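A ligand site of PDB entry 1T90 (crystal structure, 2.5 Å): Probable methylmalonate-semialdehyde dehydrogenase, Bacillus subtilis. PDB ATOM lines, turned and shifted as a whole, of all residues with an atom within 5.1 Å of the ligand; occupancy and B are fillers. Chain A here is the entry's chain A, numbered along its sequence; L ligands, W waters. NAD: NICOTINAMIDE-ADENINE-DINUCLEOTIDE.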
ATOM      1  N   ILE A 148     -27.974 -17.212 -19.083  1.00  0.00           N
ATOM      2  CA  ILE A 148     -26.750 -17.177 -18.290  1.00  0.00           C
ATOM      3  C   ILE A 148     -26.000 -15.910 -18.660  1.00  0.00           C
ATOM      4  O   ILE A 148     -25.586 -15.741 -19.802  1.00  0.00           O
ATOM      5  CB  ILE A 148     -25.908 -18.428 -18.590  1.00  0.00           C
ATOM      6  CG1 ILE A 148     -26.754 -19.684 -18.302  1.00  0.00           C
ATOM      7  CG2 ILE A 148     -24.631 -18.425 -17.758  1.00  0.00           C
ATOM      8  CD1 ILE A 148     -26.207 -20.981 -18.846  1.00  0.00           C
ATOM      9  N   ALA A 149     -25.827 -15.003 -17.692  1.00  0.00           N
ATOM     10  CA  ALA A 149     -25.176 -13.716 -17.937  1.00  0.00           C
ATOM     11  C   ALA A 149     -23.809 -13.484 -17.295  1.00  0.00           C
ATOM     12  O   ALA A 149     -23.504 -14.022 -16.240  1.00  0.00           O
ATOM     13  CB  ALA A 149     -26.134 -12.593 -17.539  1.00  0.00           C
ATOM     14  N   PRO A 150     -22.974 -12.638 -17.938  1.00  0.00           N
ATOM     15  CA  PRO A 150     -21.623 -12.282 -17.521  1.00  0.00           C
ATOM     16  C   PRO A 150     -21.589 -11.137 -16.507  1.00  0.00           C
ATOM     17  O   PRO A 150     -22.623 -10.560 -16.192  1.00  0.00           O
ATOM     18  CB  PRO A 150     -20.967 -11.884 -18.829  1.00  0.00           C
ATOM     19  CG  PRO A 150     -22.082 -11.138 -19.500  1.00  0.00           C
ATOM     20  CD  PRO A 150     -23.317 -11.974 -19.201  1.00  0.00           C
ATOM     21  N   PHE A 151     -20.395 -10.800 -16.024  1.00  0.00           N
ATOM     22  CA  PHE A 151     -20.235  -9.741 -15.033  1.00  0.00           C
ATOM     23  C   PHE A 151     -20.044  -8.330 -15.596  1.00  0.00           C
ATOM     24  O   PHE A 151     -20.328  -7.350 -14.912  1.00  0.00           O
ATOM     25  CB  PHE A 151     -19.039 -10.048 -14.119  1.00  0.00           C
ATOM     26  CG  PHE A 151     -17.725  -9.586 -14.680  1.00  0.00           C
ATOM     27  CD1 PHE A 151     -17.337  -8.244 -14.575  1.00  0.00           C
ATOM     28  CD2 PHE A 151     -16.897 -10.457 -15.386  1.00  0.00           C
ATOM     29  CE1 PHE A 151     -16.157  -7.788 -15.161  1.00  0.00           C
ATOM     30  CE2 PHE A 151     -15.709 -10.013 -15.972  1.00  0.00           C
ATOM     31  CZ  PHE A 151     -15.346  -8.670 -15.863  1.00  0.00           C
ATOM     32  N   ASN A 152     -19.552  -8.212 -16.829  1.00  0.00           N
ATOM     33  CA  ASN A 152     -19.291  -6.882 -17.371  1.00  0.00           C
ATOM     34  C   ASN A 152     -20.520  -6.006 -17.610  1.00  0.00           C
ATOM     35  O   ASN A 152     -20.391  -4.787 -17.761  1.00  0.00           O
ATOM     36  CB  ASN A 152     -18.458  -6.979 -18.657  1.00  0.00           C
ATOM     37  CG  ASN A 152     -19.179  -7.675 -19.775  1.00  0.00           C
ATOM     38  OD1 ASN A 152     -19.821  -8.692 -19.563  1.00  0.00           O
ATOM     39  ND2 ASN A 152     -19.077  -7.129 -20.976  1.00  0.00           N
ATOM     40  N   PHE A 153     -21.698  -6.618 -17.625  1.00  0.00           N
ATOM     41  CA  PHE A 153     -22.939  -5.868 -17.794  1.00  0.00           C
ATOM     42  C   PHE A 153     -24.017  -6.441 -16.895  1.00  0.00           C
ATOM     43  O   PHE A 153     -24.889  -7.174 -17.339  1.00  0.00           O
ATOM     44  CB  PHE A 153     -23.422  -5.904 -19.254  1.00  0.00           C
ATOM     45  CG  PHE A 153     -22.712  -4.922 -20.136  1.00  0.00           C
ATOM     46  CD1 PHE A 153     -21.892  -5.366 -21.173  1.00  0.00           C
ATOM     47  CD2 PHE A 153     -22.847  -3.555 -19.937  1.00  0.00           C
ATOM     48  CE1 PHE A 153     -21.227  -4.465 -22.000  1.00  0.00           C
ATOM     49  CE2 PHE A 153     -22.199  -2.640 -20.741  1.00  0.00           C
ATOM     50  CZ  PHE A 153     -21.371  -3.096 -21.779  1.00  0.00           C
ATOM     51  N   VAL A 157     -27.101  -7.009 -20.193  1.00  0.00           N
ATOM     52  CA  VAL A 157     -27.214  -8.357 -20.734  1.00  0.00           C
ATOM     53  C   VAL A 157     -28.474  -9.046 -20.238  1.00  0.00           C
ATOM     54  O   VAL A 157     -29.237  -9.589 -21.042  1.00  0.00           O
ATOM     55  CB  VAL A 157     -25.963  -9.184 -20.402  1.00  0.00           C
ATOM     56  CG1 VAL A 157     -26.179 -10.635 -20.821  1.00  0.00           C
ATOM     57  CG2 VAL A 157     -24.774  -8.587 -21.146  1.00  0.00           C
ATOM     58  N   TRP A 160     -31.372  -8.084 -22.226  1.00  0.00           N
ATOM     59  CA  TRP A 160     -31.421  -8.484 -23.643  1.00  0.00           C
ATOM     60  C   TRP A 160     -32.295  -9.727 -23.710  1.00  0.00           C
ATOM     61  O   TRP A 160     -32.957  -9.982 -24.697  1.00  0.00           O
ATOM     62  CB  TRP A 160     -30.062  -8.938 -24.189  1.00  0.00           C
ATOM     63  CG  TRP A 160     -29.007  -7.916 -24.397  1.00  0.00           C
ATOM     64  CD1 TRP A 160     -29.126  -6.564 -24.292  1.00  0.00           C
ATOM     65  CD2 TRP A 160     -27.637  -8.173 -24.763  1.00  0.00           C
ATOM     66  NE1 TRP A 160     -27.927  -5.957 -24.565  1.00  0.00           N
ATOM     67  CE2 TRP A 160     -26.998  -6.919 -24.867  1.00  0.00           C
ATOM     68  CE3 TRP A 160     -26.906  -9.337 -25.021  1.00  0.00           C
ATOM     69  CZ2 TRP A 160     -25.646  -6.797 -25.208  1.00  0.00           C
ATOM     70  CZ3 TRP A 160     -25.559  -9.227 -25.367  1.00  0.00           C
ATOM     71  CH2 TRP A 160     -24.942  -7.953 -25.456  1.00  0.00           C
ATOM     72  N   LYS A 175     -29.675 -17.004 -14.655  1.00  0.00           N
ATOM     73  CA  LYS A 175     -28.552 -17.284 -13.770  1.00  0.00           C
ATOM     74  C   LYS A 175     -27.557 -16.166 -14.021  1.00  0.00           C
ATOM     75  O   LYS A 175     -26.718 -16.273 -14.920  1.00  0.00           O
ATOM     76  CB  LYS A 175     -27.877 -18.622 -14.105  1.00  0.00           C
ATOM     77  CG  LYS A 175     -26.930 -19.086 -12.995  1.00  0.00           C
ATOM     78  CD  LYS A 175     -25.663 -19.729 -13.534  1.00  0.00           C
ATOM     79  CE  LYS A 175     -24.687 -18.686 -14.084  1.00  0.00           C
ATOM     80  NZ  LYS A 175     -24.147 -17.771 -13.020  1.00  0.00           N
ATOM     81  N   PRO A 176     -27.634 -15.072 -13.254  1.00  0.00           N
ATOM     82  CA  PRO A 176     -26.716 -13.946 -13.432  1.00  0.00           C
ATOM     83  C   PRO A 176     -25.302 -14.279 -13.002  1.00  0.00           C
ATOM     84  O   PRO A 176     -25.028 -15.361 -12.486  1.00  0.00           O
ATOM     85  CB  PRO A 176     -27.340 -12.860 -12.564  1.00  0.00           C
ATOM     86  CG  PRO A 176     -27.924 -13.654 -11.443  1.00  0.00           C
ATOM     87  CD  PRO A 176     -28.569 -14.832 -12.133  1.00  0.00           C
ATOM     88  N   SER A 177     -24.378 -13.362 -13.240  1.00  0.00           N
ATOM     89  CA  SER A 177     -22.995 -13.606 -12.850  1.00  0.00           C
ATOM     90  C   SER A 177     -22.904 -13.680 -11.344  1.00  0.00           C
ATOM     91  O   SER A 177     -23.540 -12.911 -10.632  1.00  0.00           O
ATOM     92  CB  SER A 177     -22.086 -12.480 -13.334  1.00  0.00           C
ATOM     93  OG  SER A 177     -20.829 -12.551 -12.672  1.00  0.00           O
ATOM     94  N   GLU A 178     -22.082 -14.607 -10.863  1.00  0.00           N
ATOM     95  CA  GLU A 178     -21.891 -14.794  -9.424  1.00  0.00           C
ATOM     96  C   GLU A 178     -21.230 -13.553  -8.814  1.00  0.00           C
ATOM     97  O   GLU A 178     -21.374 -13.293  -7.624  1.00  0.00           O
ATOM     98  CB  GLU A 178     -21.029 -16.044  -9.168  1.00  0.00           C
ATOM     99  CG  GLU A 178     -19.641 -16.080  -9.879  1.00  0.00           C
ATOM    100  CD  GLU A 178     -19.686 -16.503 -11.358  1.00  0.00           C
ATOM    101  OE1 GLU A 178     -20.507 -17.388 -11.680  1.00  0.00           O
ATOM    102  OE2 GLU A 178     -18.892 -15.992 -12.180  1.00  0.00           O
ATOM    103  N   ARG A 179     -20.523 -12.787  -9.640  1.00  0.00           N
ATOM    104  CA  ARG A 179     -19.832 -11.595  -9.173  1.00  0.00           C
ATOM    105  C   ARG A 179     -20.674 -10.321  -9.111  1.00  0.00           C
ATOM    106  O   ARG A 179     -20.375  -9.433  -8.315  1.00  0.00           O
ATOM    107  CB  ARG A 179     -18.588 -11.353 -10.048  1.00  0.00           C
ATOM    108  CG  ARG A 179     -17.470 -12.339  -9.756  1.00  0.00           C
ATOM    109  CD  ARG A 179     -16.313 -12.207 -10.711  1.00  0.00           C
ATOM    110  NE  ARG A 179     -16.588 -12.834 -11.999  1.00  0.00           N
ATOM    111  CZ  ARG A 179     -15.692 -12.938 -12.977  1.00  0.00           C
ATOM    112  NH1 ARG A 179     -14.464 -12.453 -12.821  1.00  0.00           N
ATOM    113  NH2 ARG A 179     -16.014 -13.544 -14.119  1.00  0.00           N
ATOM    114  N   GLY A 206     -25.818 -18.907  -8.744  1.00  0.00           N
ATOM    115  CA  GLY A 206     -24.927 -20.046  -8.652  1.00  0.00           C
ATOM    116  C   GLY A 206     -23.803 -20.065  -9.667  1.00  0.00           C
ATOM    117  O   GLY A 206     -23.428 -19.033 -10.211  1.00  0.00           O
ATOM    118  N   ALA A 207     -23.267 -21.257  -9.898  1.00  0.00           N
ATOM    119  CA  ALA A 207     -22.181 -21.420 -10.852  1.00  0.00           C
ATOM    120  C   ALA A 207     -22.426 -22.621 -11.762  1.00  0.00           C
ATOM    121  O   ALA A 207     -23.405 -22.660 -12.499  1.00  0.00           O
ATOM    122  CB  ALA A 207     -20.866 -21.571 -10.103  1.00  0.00           C
ATOM    123  N   HIS A 208     -21.538 -23.617 -11.690  1.00  0.00           N
ATOM    124  CA  HIS A 208     -21.636 -24.787 -12.550  1.00  0.00           C
ATOM    125  C   HIS A 208     -22.841 -25.697 -12.356  1.00  0.00           C
ATOM    126  O   HIS A 208     -23.513 -26.026 -13.335  1.00  0.00           O
ATOM    127  CB  HIS A 208     -20.355 -25.612 -12.437  1.00  0.00           C
ATOM    128  CG  HIS A 208     -19.118 -24.852 -12.808  1.00  0.00           C
ATOM    129  ND1 HIS A 208     -17.894 -25.463 -13.009  1.00  0.00           N
ATOM    130  CD2 HIS A 208     -18.910 -23.522 -12.986  1.00  0.00           C
ATOM    131  CE1 HIS A 208     -16.983 -24.538 -13.289  1.00  0.00           C
ATOM    132  NE2 HIS A 208     -17.579 -23.354 -13.279  1.00  0.00           N
ATOM    133  N   VAL A 211     -25.687 -24.101 -14.079  1.00  0.00           N
ATOM    134  CA  VAL A 211     -25.551 -23.968 -15.526  1.00  0.00           C
ATOM    135  C   VAL A 211     -25.759 -25.305 -16.207  1.00  0.00           C
ATOM    136  O   VAL A 211     -26.437 -25.384 -17.237  1.00  0.00           O
ATOM    137  CB  VAL A 211     -24.163 -23.388 -15.922  1.00  0.00           C
ATOM    138  CG1 VAL A 211     -23.969 -23.464 -17.421  1.00  0.00           C
ATOM    139  CG2 VAL A 211     -24.058 -21.944 -15.474  1.00  0.00           C
ATOM    140  N   PHE A 225     -26.718 -17.728 -23.863  1.00  0.00           N
ATOM    141  CA  PHE A 225     -25.482 -17.592 -23.102  1.00  0.00           C
ATOM    142  C   PHE A 225     -24.694 -16.394 -23.578  1.00  0.00           C
ATOM    143  O   PHE A 225     -24.514 -16.204 -24.786  1.00  0.00           O
ATOM    144  CB  PHE A 225     -24.593 -18.827 -23.224  1.00  0.00           C
ATOM    145  CG  PHE A 225     -23.238 -18.655 -22.604  1.00  0.00           C
ATOM    146  CD1 PHE A 225     -23.014 -18.972 -21.257  1.00  0.00           C
ATOM    147  CD2 PHE A 225     -22.180 -18.093 -23.327  1.00  0.00           C
ATOM    148  CE1 PHE A 225     -21.775 -18.741 -20.656  1.00  0.00           C
ATOM    149  CE2 PHE A 225     -20.934 -17.858 -22.742  1.00  0.00           C
ATOM    150  CZ  PHE A 225     -20.732 -18.182 -21.400  1.00  0.00           C
ATOM    151  N   VAL A 226     -24.201 -15.622 -22.617  1.00  0.00           N
ATOM    152  CA  VAL A 226     -23.394 -14.451 -22.900  1.00  0.00           C
ATOM    153  C   VAL A 226     -22.178 -14.489 -21.956  1.00  0.00           C
ATOM    154  O   VAL A 226     -22.318 -14.286 -20.755  1.00  0.00           O
ATOM    155  CB  VAL A 226     -24.198 -13.150 -22.674  1.00  0.00           C
ATOM    156  CG1 VAL A 226     -23.360 -11.951 -23.013  1.00  0.00           C
ATOM    157  CG2 VAL A 226     -25.466 -13.155 -23.528  1.00  0.00           C
ATOM    158  N   GLY A 227     -21.000 -14.783 -22.502  1.00  0.00           N
ATOM    159  CA  GLY A 227     -19.791 -14.870 -21.703  1.00  0.00           C
ATOM    160  C   GLY A 227     -18.533 -15.103 -22.515  1.00  0.00           C
ATOM    161  O   GLY A 227     -18.484 -14.746 -23.692  1.00  0.00           O
ATOM    162  N   SER A 228     -17.512 -15.708 -21.902  1.00  0.00           N
ATOM    163  CA  SER A 228     -16.229 -15.993 -22.570  1.00  0.00           C
ATOM    164  C   SER A 228     -16.360 -17.067 -23.649  1.00  0.00           C
ATOM    165  O   SER A 228     -17.252 -17.904 -23.601  1.00  0.00           O
ATOM    166  CB  SER A 228     -15.210 -16.460 -21.540  1.00  0.00           C
ATOM    167  OG  SER A 228     -15.498 -17.783 -21.116  1.00  0.00           O
ATOM    168  N   LYS A 229     -15.447 -17.048 -24.619  1.00  0.00           N
ATOM    169  CA  LYS A 229     -15.472 -18.026 -25.700  1.00  0.00           C
ATOM    170  C   LYS A 229     -15.421 -19.470 -25.201  1.00  0.00           C
ATOM    171  O   LYS A 229     -16.193 -20.298 -25.642  1.00  0.00           O
ATOM    172  CB  LYS A 229     -14.329 -17.810 -26.682  1.00  0.00           C
ATOM    173  CG  LYS A 229     -14.163 -18.957 -27.678  1.00  0.00           C
ATOM    174  CD  LYS A 229     -13.174 -18.632 -28.772  1.00  0.00           C
ATOM    175  CE  LYS A 229     -12.919 -19.830 -29.668  1.00  0.00           C
ATOM    176  NZ  LYS A 229     -12.136 -20.893 -28.975  1.00  0.00           N
ATOM    177  N   VAL A 231     -16.261 -20.892 -22.250  1.00  0.00           N
ATOM    178  CA  VAL A 231     -17.513 -21.302 -21.623  1.00  0.00           C
ATOM    179  C   VAL A 231     -18.670 -21.362 -22.608  1.00  0.00           C
ATOM    180  O   VAL A 231     -19.466 -22.296 -22.585  1.00  0.00           O
ATOM    181  CB  VAL A 231     -17.910 -20.352 -20.486  1.00  0.00           C
ATOM    182  CG1 VAL A 231     -19.148 -20.872 -19.793  1.00  0.00           C
ATOM    183  CG2 VAL A 231     -16.754 -20.234 -19.499  1.00  0.00           C
ATOM    184  N   TYR A 234     -18.521 -24.267 -24.957  1.00  0.00           N
ATOM    185  CA  TYR A 234     -18.988 -25.436 -24.224  1.00  0.00           C
ATOM    186  C   TYR A 234     -20.518 -25.466 -24.105  1.00  0.00           C
ATOM    187  O   TYR A 234     -21.148 -26.495 -24.381  1.00  0.00           O
ATOM    188  CB  TYR A 234     -18.343 -25.462 -22.837  1.00  0.00           C
ATOM    189  CG  TYR A 234     -19.015 -26.375 -21.829  1.00  0.00           C
ATOM    190  CD1 TYR A 234     -19.898 -25.863 -20.883  1.00  0.00           C
ATOM    191  CD2 TYR A 234     -18.751 -27.748 -21.822  1.00  0.00           C
ATOM    192  CE1 TYR A 234     -20.508 -26.684 -19.935  1.00  0.00           C
ATOM    193  CE2 TYR A 234     -19.364 -28.588 -20.886  1.00  0.00           C
ATOM    194  CZ  TYR A 234     -20.238 -28.053 -19.944  1.00  0.00           C
ATOM    195  OH  TYR A 234     -20.839 -28.876 -19.018  1.00  0.00           O
ATOM    196  N   LEU A 249     -23.124 -15.653 -27.269  1.00  0.00           N
ATOM    197  CA  LEU A 249     -22.472 -14.408 -27.660  1.00  0.00           C
ATOM    198  C   LEU A 249     -21.202 -14.427 -26.811  1.00  0.00           C
ATOM    199  O   LEU A 249     -21.234 -14.203 -25.611  1.00  0.00           O
ATOM    200  CB  LEU A 249     -23.352 -13.200 -27.323  1.00  0.00           C
ATOM    201  CG  LEU A 249     -24.437 -12.913 -28.370  1.00  0.00           C
ATOM    202  CD1 LEU A 249     -25.361 -14.113 -28.485  1.00  0.00           C
ATOM    203  CD2 LEU A 249     -25.222 -11.675 -28.005  1.00  0.00           C
ATOM    204  N   THR A 250     -20.074 -14.697 -27.474  1.00  0.00           N
ATOM    205  CA  THR A 250     -18.811 -14.841 -26.784  1.00  0.00           C
ATOM    206  C   THR A 250     -17.771 -13.717 -26.835  1.00  0.00           C
ATOM    207  O   THR A 250     -18.101 -12.535 -27.038  1.00  0.00           O
ATOM    208  CB  THR A 250     -18.153 -16.148 -27.227  1.00  0.00           C
ATOM    209  OG1 THR A 250     -17.985 -16.130 -28.654  1.00  0.00           O
ATOM    210  CG2 THR A 250     -19.051 -17.328 -26.875  1.00  0.00           C
ATOM    211  N   GLY A 251     -16.514 -14.098 -26.631  1.00  0.00           N
ATOM    212  CA  GLY A 251     -15.395 -13.159 -26.602  1.00  0.00           C
ATOM    213  C   GLY A 251     -15.166 -12.256 -27.796  1.00  0.00           C
ATOM    214  O   GLY A 251     -15.788 -12.407 -28.848  1.00  0.00           O
ATOM    215  N   ALA A 252     -14.252 -11.300 -27.628  1.00  0.00           N
ATOM    216  CA  ALA A 252     -13.946 -10.344 -28.679  1.00  0.00           C
ATOM    217  C   ALA A 252     -12.513  -9.832 -28.630  1.00  0.00           C
ATOM    218  O   ALA A 252     -11.786 -10.002 -27.648  1.00  0.00           O
ATOM    219  CB  ALA A 252     -14.893  -9.164 -28.603  1.00  0.00           C
ATOM    220  N   CYS A 283     -17.370  -6.396 -24.297  1.00  0.00           N
ATOM    221  CA  CYS A 283     -17.316  -7.186 -25.519  1.00  0.00           C
ATOM    222  C   CYS A 283     -17.152  -6.257 -26.707  1.00  0.00           C
ATOM    223  O   CYS A 283     -16.775  -6.675 -27.804  1.00  0.00           O
ATOM    224  CB  CYS A 283     -18.615  -7.982 -25.674  1.00  0.00           C
ATOM    225  SG  CYS A 283     -20.103  -6.978 -25.469  1.00  0.00           S
ATOM    226  N   GLU A 381      -7.904 -12.195 -25.657  1.00  0.00           N
ATOM    227  CA  GLU A 381      -8.738 -11.108 -25.186  1.00  0.00           C
ATOM    228  C   GLU A 381      -8.229 -10.800 -23.783  1.00  0.00           C
ATOM    229  O   GLU A 381      -8.454 -11.567 -22.861  1.00  0.00           O
ATOM    230  CB  GLU A 381     -10.204 -11.555 -25.108  1.00  0.00           C
ATOM    231  CG  GLU A 381     -11.167 -10.412 -24.861  1.00  0.00           C
ATOM    232  CD  GLU A 381     -12.614 -10.871 -24.735  1.00  0.00           C
ATOM    233  OE1 GLU A 381     -13.521 -10.034 -24.954  1.00  0.00           O
ATOM    234  OE2 GLU A 381     -12.845 -12.055 -24.417  1.00  0.00           O
ATOM    235  N   PHE A 383      -9.182  -8.320 -22.036  1.00  0.00           N
ATOM    236  CA  PHE A 383     -10.386  -7.922 -21.325  1.00  0.00           C
ATOM    237  C   PHE A 383     -10.035  -7.100 -20.100  1.00  0.00           C
ATOM    238  O   PHE A 383     -10.531  -7.340 -18.998  1.00  0.00           O
ATOM    239  CB  PHE A 383     -11.197  -9.162 -20.921  1.00  0.00           C
ATOM    240  CG  PHE A 383     -12.666  -8.922 -20.813  1.00  0.00           C
ATOM    241  CD1 PHE A 383     -13.302  -8.931 -19.572  1.00  0.00           C
ATOM    242  CD2 PHE A 383     -13.424  -8.620 -21.947  1.00  0.00           C
ATOM    243  CE1 PHE A 383     -14.663  -8.652 -19.467  1.00  0.00           C
ATOM    244  CE2 PHE A 383     -14.774  -8.342 -21.850  1.00  0.00           C
ATOM    245  CZ  PHE A 383     -15.405  -8.357 -20.602  1.00  0.00           C
ATOM    246  N   ASN A 409     -16.442  -9.699 -33.331  1.00  0.00           N
ATOM    247  CA  ASN A 409     -17.630  -9.147 -32.700  1.00  0.00           C
ATOM    248  C   ASN A 409     -17.877  -7.766 -33.297  1.00  0.00           C
ATOM    249  O   ASN A 409     -18.850  -7.555 -34.023  1.00  0.00           O
ATOM    250  CB  ASN A 409     -17.457  -9.029 -31.180  1.00  0.00           C
ATOM    251  CG  ASN A 409     -18.777  -9.178 -30.439  1.00  0.00           C
ATOM    252  OD1 ASN A 409     -18.940  -8.676 -29.327  1.00  0.00           O
ATOM    253  ND2 ASN A 409     -19.714  -9.896 -31.041  1.00  0.00           N
ATOM    254  N   PHE A 448     -27.841  -7.934 -32.332  1.00  0.00           N
ATOM    255  CA  PHE A 448     -26.455  -7.767 -31.880  1.00  0.00           C
ATOM    256  C   PHE A 448     -25.593  -8.744 -32.716  1.00  0.00           C
ATOM    257  O   PHE A 448     -25.114  -9.748 -32.198  1.00  0.00           O
ATOM    258  CB  PHE A 448     -26.392  -8.133 -30.401  1.00  0.00           C
ATOM    259  CG  PHE A 448     -25.300  -7.437 -29.638  1.00  0.00           C
ATOM    260  CD1 PHE A 448     -25.470  -6.117 -29.209  1.00  0.00           C
ATOM    261  CD2 PHE A 448     -24.116  -8.096 -29.321  1.00  0.00           C
ATOM    262  CE1 PHE A 448     -24.470  -5.475 -28.479  1.00  0.00           C
ATOM    263  CE2 PHE A 448     -23.104  -7.472 -28.584  1.00  0.00           C
ATOM    264  CZ  PHE A 448     -23.278  -6.146 -28.162  1.00  0.00           C
ATOM    265  N   SER A 454     -16.857 -15.189 -31.919  1.00  0.00           N
ATOM    266  CA  SER A 454     -17.592 -14.255 -31.074  1.00  0.00           C
ATOM    267  C   SER A 454     -19.067 -14.631 -30.994  1.00  0.00           C
ATOM    268  O   SER A 454     -19.789 -14.156 -30.102  1.00  0.00           O
ATOM    269  CB  SER A 454     -17.440 -12.828 -31.597  1.00  0.00           C
ATOM    270  OG  SER A 454     -16.099 -12.396 -31.544  1.00  0.00           O
HETATM  271  PA  NAD L   1     -17.469 -16.260 -18.156  1.00  0.00           P
HETATM  272  O1A NAD L   1     -17.661 -17.069 -19.396  1.00  0.00           O
HETATM  273  O2A NAD L   1     -16.343 -16.426 -17.175  1.00  0.00           O
HETATM  274  O5B NAD L   1     -18.798 -16.312 -17.252  1.00  0.00           O
HETATM  275  C5B NAD L   1     -20.087 -15.946 -17.873  1.00  0.00           C
HETATM  276  C4B NAD L   1     -21.175 -16.860 -17.263  1.00  0.00           C
HETATM  277  O4B NAD L   1     -20.633 -18.217 -17.465  1.00  0.00           O
HETATM  278  C3B NAD L   1     -21.259 -16.591 -15.724  1.00  0.00           C
HETATM  279  O3B NAD L   1     -22.687 -16.508 -15.377  1.00  0.00           O
HETATM  280  C2B NAD L   1     -20.606 -17.835 -15.134  1.00  0.00           C
HETATM  281  O2B NAD L   1     -21.135 -18.267 -13.924  1.00  0.00           O
HETATM  282  C1B NAD L   1     -20.648 -18.935 -16.223  1.00  0.00           C
HETATM  283  N9A NAD L   1     -19.440 -19.708 -16.248  1.00  0.00           N
HETATM  284  C8A NAD L   1     -18.075 -19.370 -16.210  1.00  0.00           C
HETATM  285  N7A NAD L   1     -17.278 -20.429 -16.264  1.00  0.00           N
HETATM  286  C5A NAD L   1     -18.066 -21.529 -16.341  1.00  0.00           C
HETATM  287  C6A NAD L   1     -17.784 -22.975 -16.430  1.00  0.00           C
HETATM  288  N6A NAD L   1     -16.562 -23.458 -16.449  1.00  0.00           N
HETATM  289  N1A NAD L   1     -18.915 -23.778 -16.491  1.00  0.00           N
HETATM  290  C2A NAD L   1     -20.185 -23.353 -16.483  1.00  0.00           C
HETATM  291  N3A NAD L   1     -20.508 -21.994 -16.402  1.00  0.00           N
HETATM  292  C4A NAD L   1     -19.415 -21.114 -16.329  1.00  0.00           C
HETATM  293  O3  NAD L   1     -17.421 -14.714 -18.548  1.00  0.00           O
HETATM  294  PN  NAD L   1     -17.243 -13.320 -17.690  1.00  0.00           P
HETATM  295  O1N NAD L   1     -15.832 -13.187 -17.238  1.00  0.00           O
HETATM  296  O2N NAD L   1     -18.263 -13.359 -16.590  1.00  0.00           O
HETATM  297  O5D NAD L   1     -17.555 -12.165 -18.795  1.00  0.00           O
HETATM  298  C5D NAD L   1     -16.496 -11.647 -19.665  1.00  0.00           C
HETATM  299  C4D NAD L   1     -16.572 -12.354 -20.964  1.00  0.00           C
HETATM  300  O4D NAD L   1     -17.956 -12.214 -21.531  1.00  0.00           O
HETATM  301  C3D NAD L   1     -15.624 -11.776 -22.084  1.00  0.00           C
HETATM  302  O3D NAD L   1     -14.979 -12.838 -22.820  1.00  0.00           O
HETATM  303  C2D NAD L   1     -16.571 -10.961 -22.976  1.00  0.00           C
HETATM  304  O2D NAD L   1     -16.068 -10.751 -24.276  1.00  0.00           O
HETATM  305  C1D NAD L   1     -17.890 -11.812 -22.915  1.00  0.00           C
HETATM  306  N1N NAD L   1     -19.130 -11.055 -23.306  1.00  0.00           N
HETATM  307  C2N NAD L   1     -19.718 -11.168 -24.624  1.00  0.00           C
HETATM  308  C3N NAD L   1     -20.783 -10.412 -24.937  1.00  0.00           C
HETATM  309  C7N NAD L   1     -21.399 -10.520 -26.316  1.00  0.00           C
HETATM  310  O7N NAD L   1     -22.634 -10.293 -26.437  1.00  0.00           O
HETATM  311  N7N NAD L   1     -20.625 -10.859 -27.357  1.00  0.00           N
HETATM  312  C4N NAD L   1     -21.385  -9.430 -23.934  1.00  0.00           C
HETATM  313  C5N NAD L   1     -20.773  -9.393 -22.563  1.00  0.00           C
HETATM  314  C6N NAD L   1     -19.642 -10.182 -22.276  1.00  0.00           C
HETATM  315  O   HOH W   1     -21.393 -11.851 -30.031  1.00  0.00           O
HETATM  316  O   HOH W   2     -19.419 -14.494 -14.291  1.00  0.00           O
HETATM  317  O   HOH W   3     -18.946 -26.794 -16.195  1.00  0.00           O
HETATM  318  O   HOH W   4     -13.402 -14.806 -24.543  1.00  0.00           O
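The side-chain carboxylate of Glu 178 is in hydrogen-bond range of an oxygen (O2B) of the ligand (2.5 Å). The side-chain carboxylate (OE1) of Glu 381 is in hydrogen-bond range of an oxygen (O2D) of the ligand (2.7 Å). The backbone carbonyl oxygen (O) of Ala 149 lies within hydrogen-bond range of an oxygen (O3B) of the ligand (2.8 Å). The backbone NH (N) of Ser 228 sits at hydrogen-bond distance from an oxygen (O1A) of the ligand (2.9 Å). The side-chain hydroxyl of Ser 228 lies within hydrogen-bond range of an oxygen (O1A) of the ligand. A nitrogen (N7N) of the ligand is in hydrogen-bond range of the backbone carbonyl oxygen of Thr 250. An oxygen (O3B) of the ligand sits at hydrogen-bond distance from the side-chain amino group of Lys 175, at 3.0 Å. An oxygen (O1N) of the ligand is in salt-bridge range of the guanidinium group (NH2) of Arg 179. NE2 of His 208 lies close to N6A of the ligand. N of Phe 151 is in hydrogen-bond range of O2N of the ligand (3.4 Å). OD1 of Asn 409 is in hydrogen-bond range of N7N of the ligand, at 3.4 Å.
The backbone NH of Ala 252 lies within hydrogen-bond range of the side-chain carboxylate of Glu 381 (3.0 Å). N of Val 231 sits close to OG of Ser 228 (3.4 Å). O of Ser 454 sits at hydrogen-bond distance from N of Thr 250 (2.7 Å). The side-chain amino group (NZ) of Lys 175 sits at hydrogen-bond distance from the backbone carbonyl oxygen (O) of Gly 206, 3.2 Å away. N of Arg 179 lies within hydrogen-bond range of OG of Ser 177 (3.1 Å). OD1 of Asn 409 lies close to O of Cys 283 (3.3 Å). The backbone NH (N) of Val 226 lies within hydrogen-bond range of the backbone carbonyl oxygen (O) of Ile 148 (3.1 Å). OG of Ser 454 sits at hydrogen-bond distance from O of Gly 251 (2.7 Å).
O4D of the ligand sits close to O of Gly 227 (3.4 Å). Merely in contact with the ligand: Asn 152, Leu 249, Cys 283, Val 231, Trp 160, Val 226, Phe 383, Gly 251, Pro 150, Phe 225, Phe 448, Ile 148, Val 211, Ala 252, Ser 177 and Pro 176. Hydrophobic or aromatic side chains within 4 Å of the ligand: Ile 148, Pro 150, Phe 151, Trp 160, His 208, Val 211, Phe 225, Val 226, Val 231, Leu 249, Phe 383 and Phe 448. Of the 34 residues printed, 27 come within 4 Å of the ligand. The nearest printed residue that does not touch the ligand is Val 157 (4.3 Å).
Water W2 lies within hydrogen-bond range of OE2 of Glu 178 (2.6 Å), O2N of the ligand (2.8 Å) and OG of Ser 177 (2.9 Å). Water W1 lies within hydrogen-bond range of ND2 of Asn 409, O of Ser 454 and N7N of the ligand. Water W4 lies within hydrogen-bond range of the side-chain carboxylate of Glu 381 (2.8 Å), the backbone NH of Lys 229 (3.0 Å) and an oxygen (O3D) of the ligand (3.1 Å).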
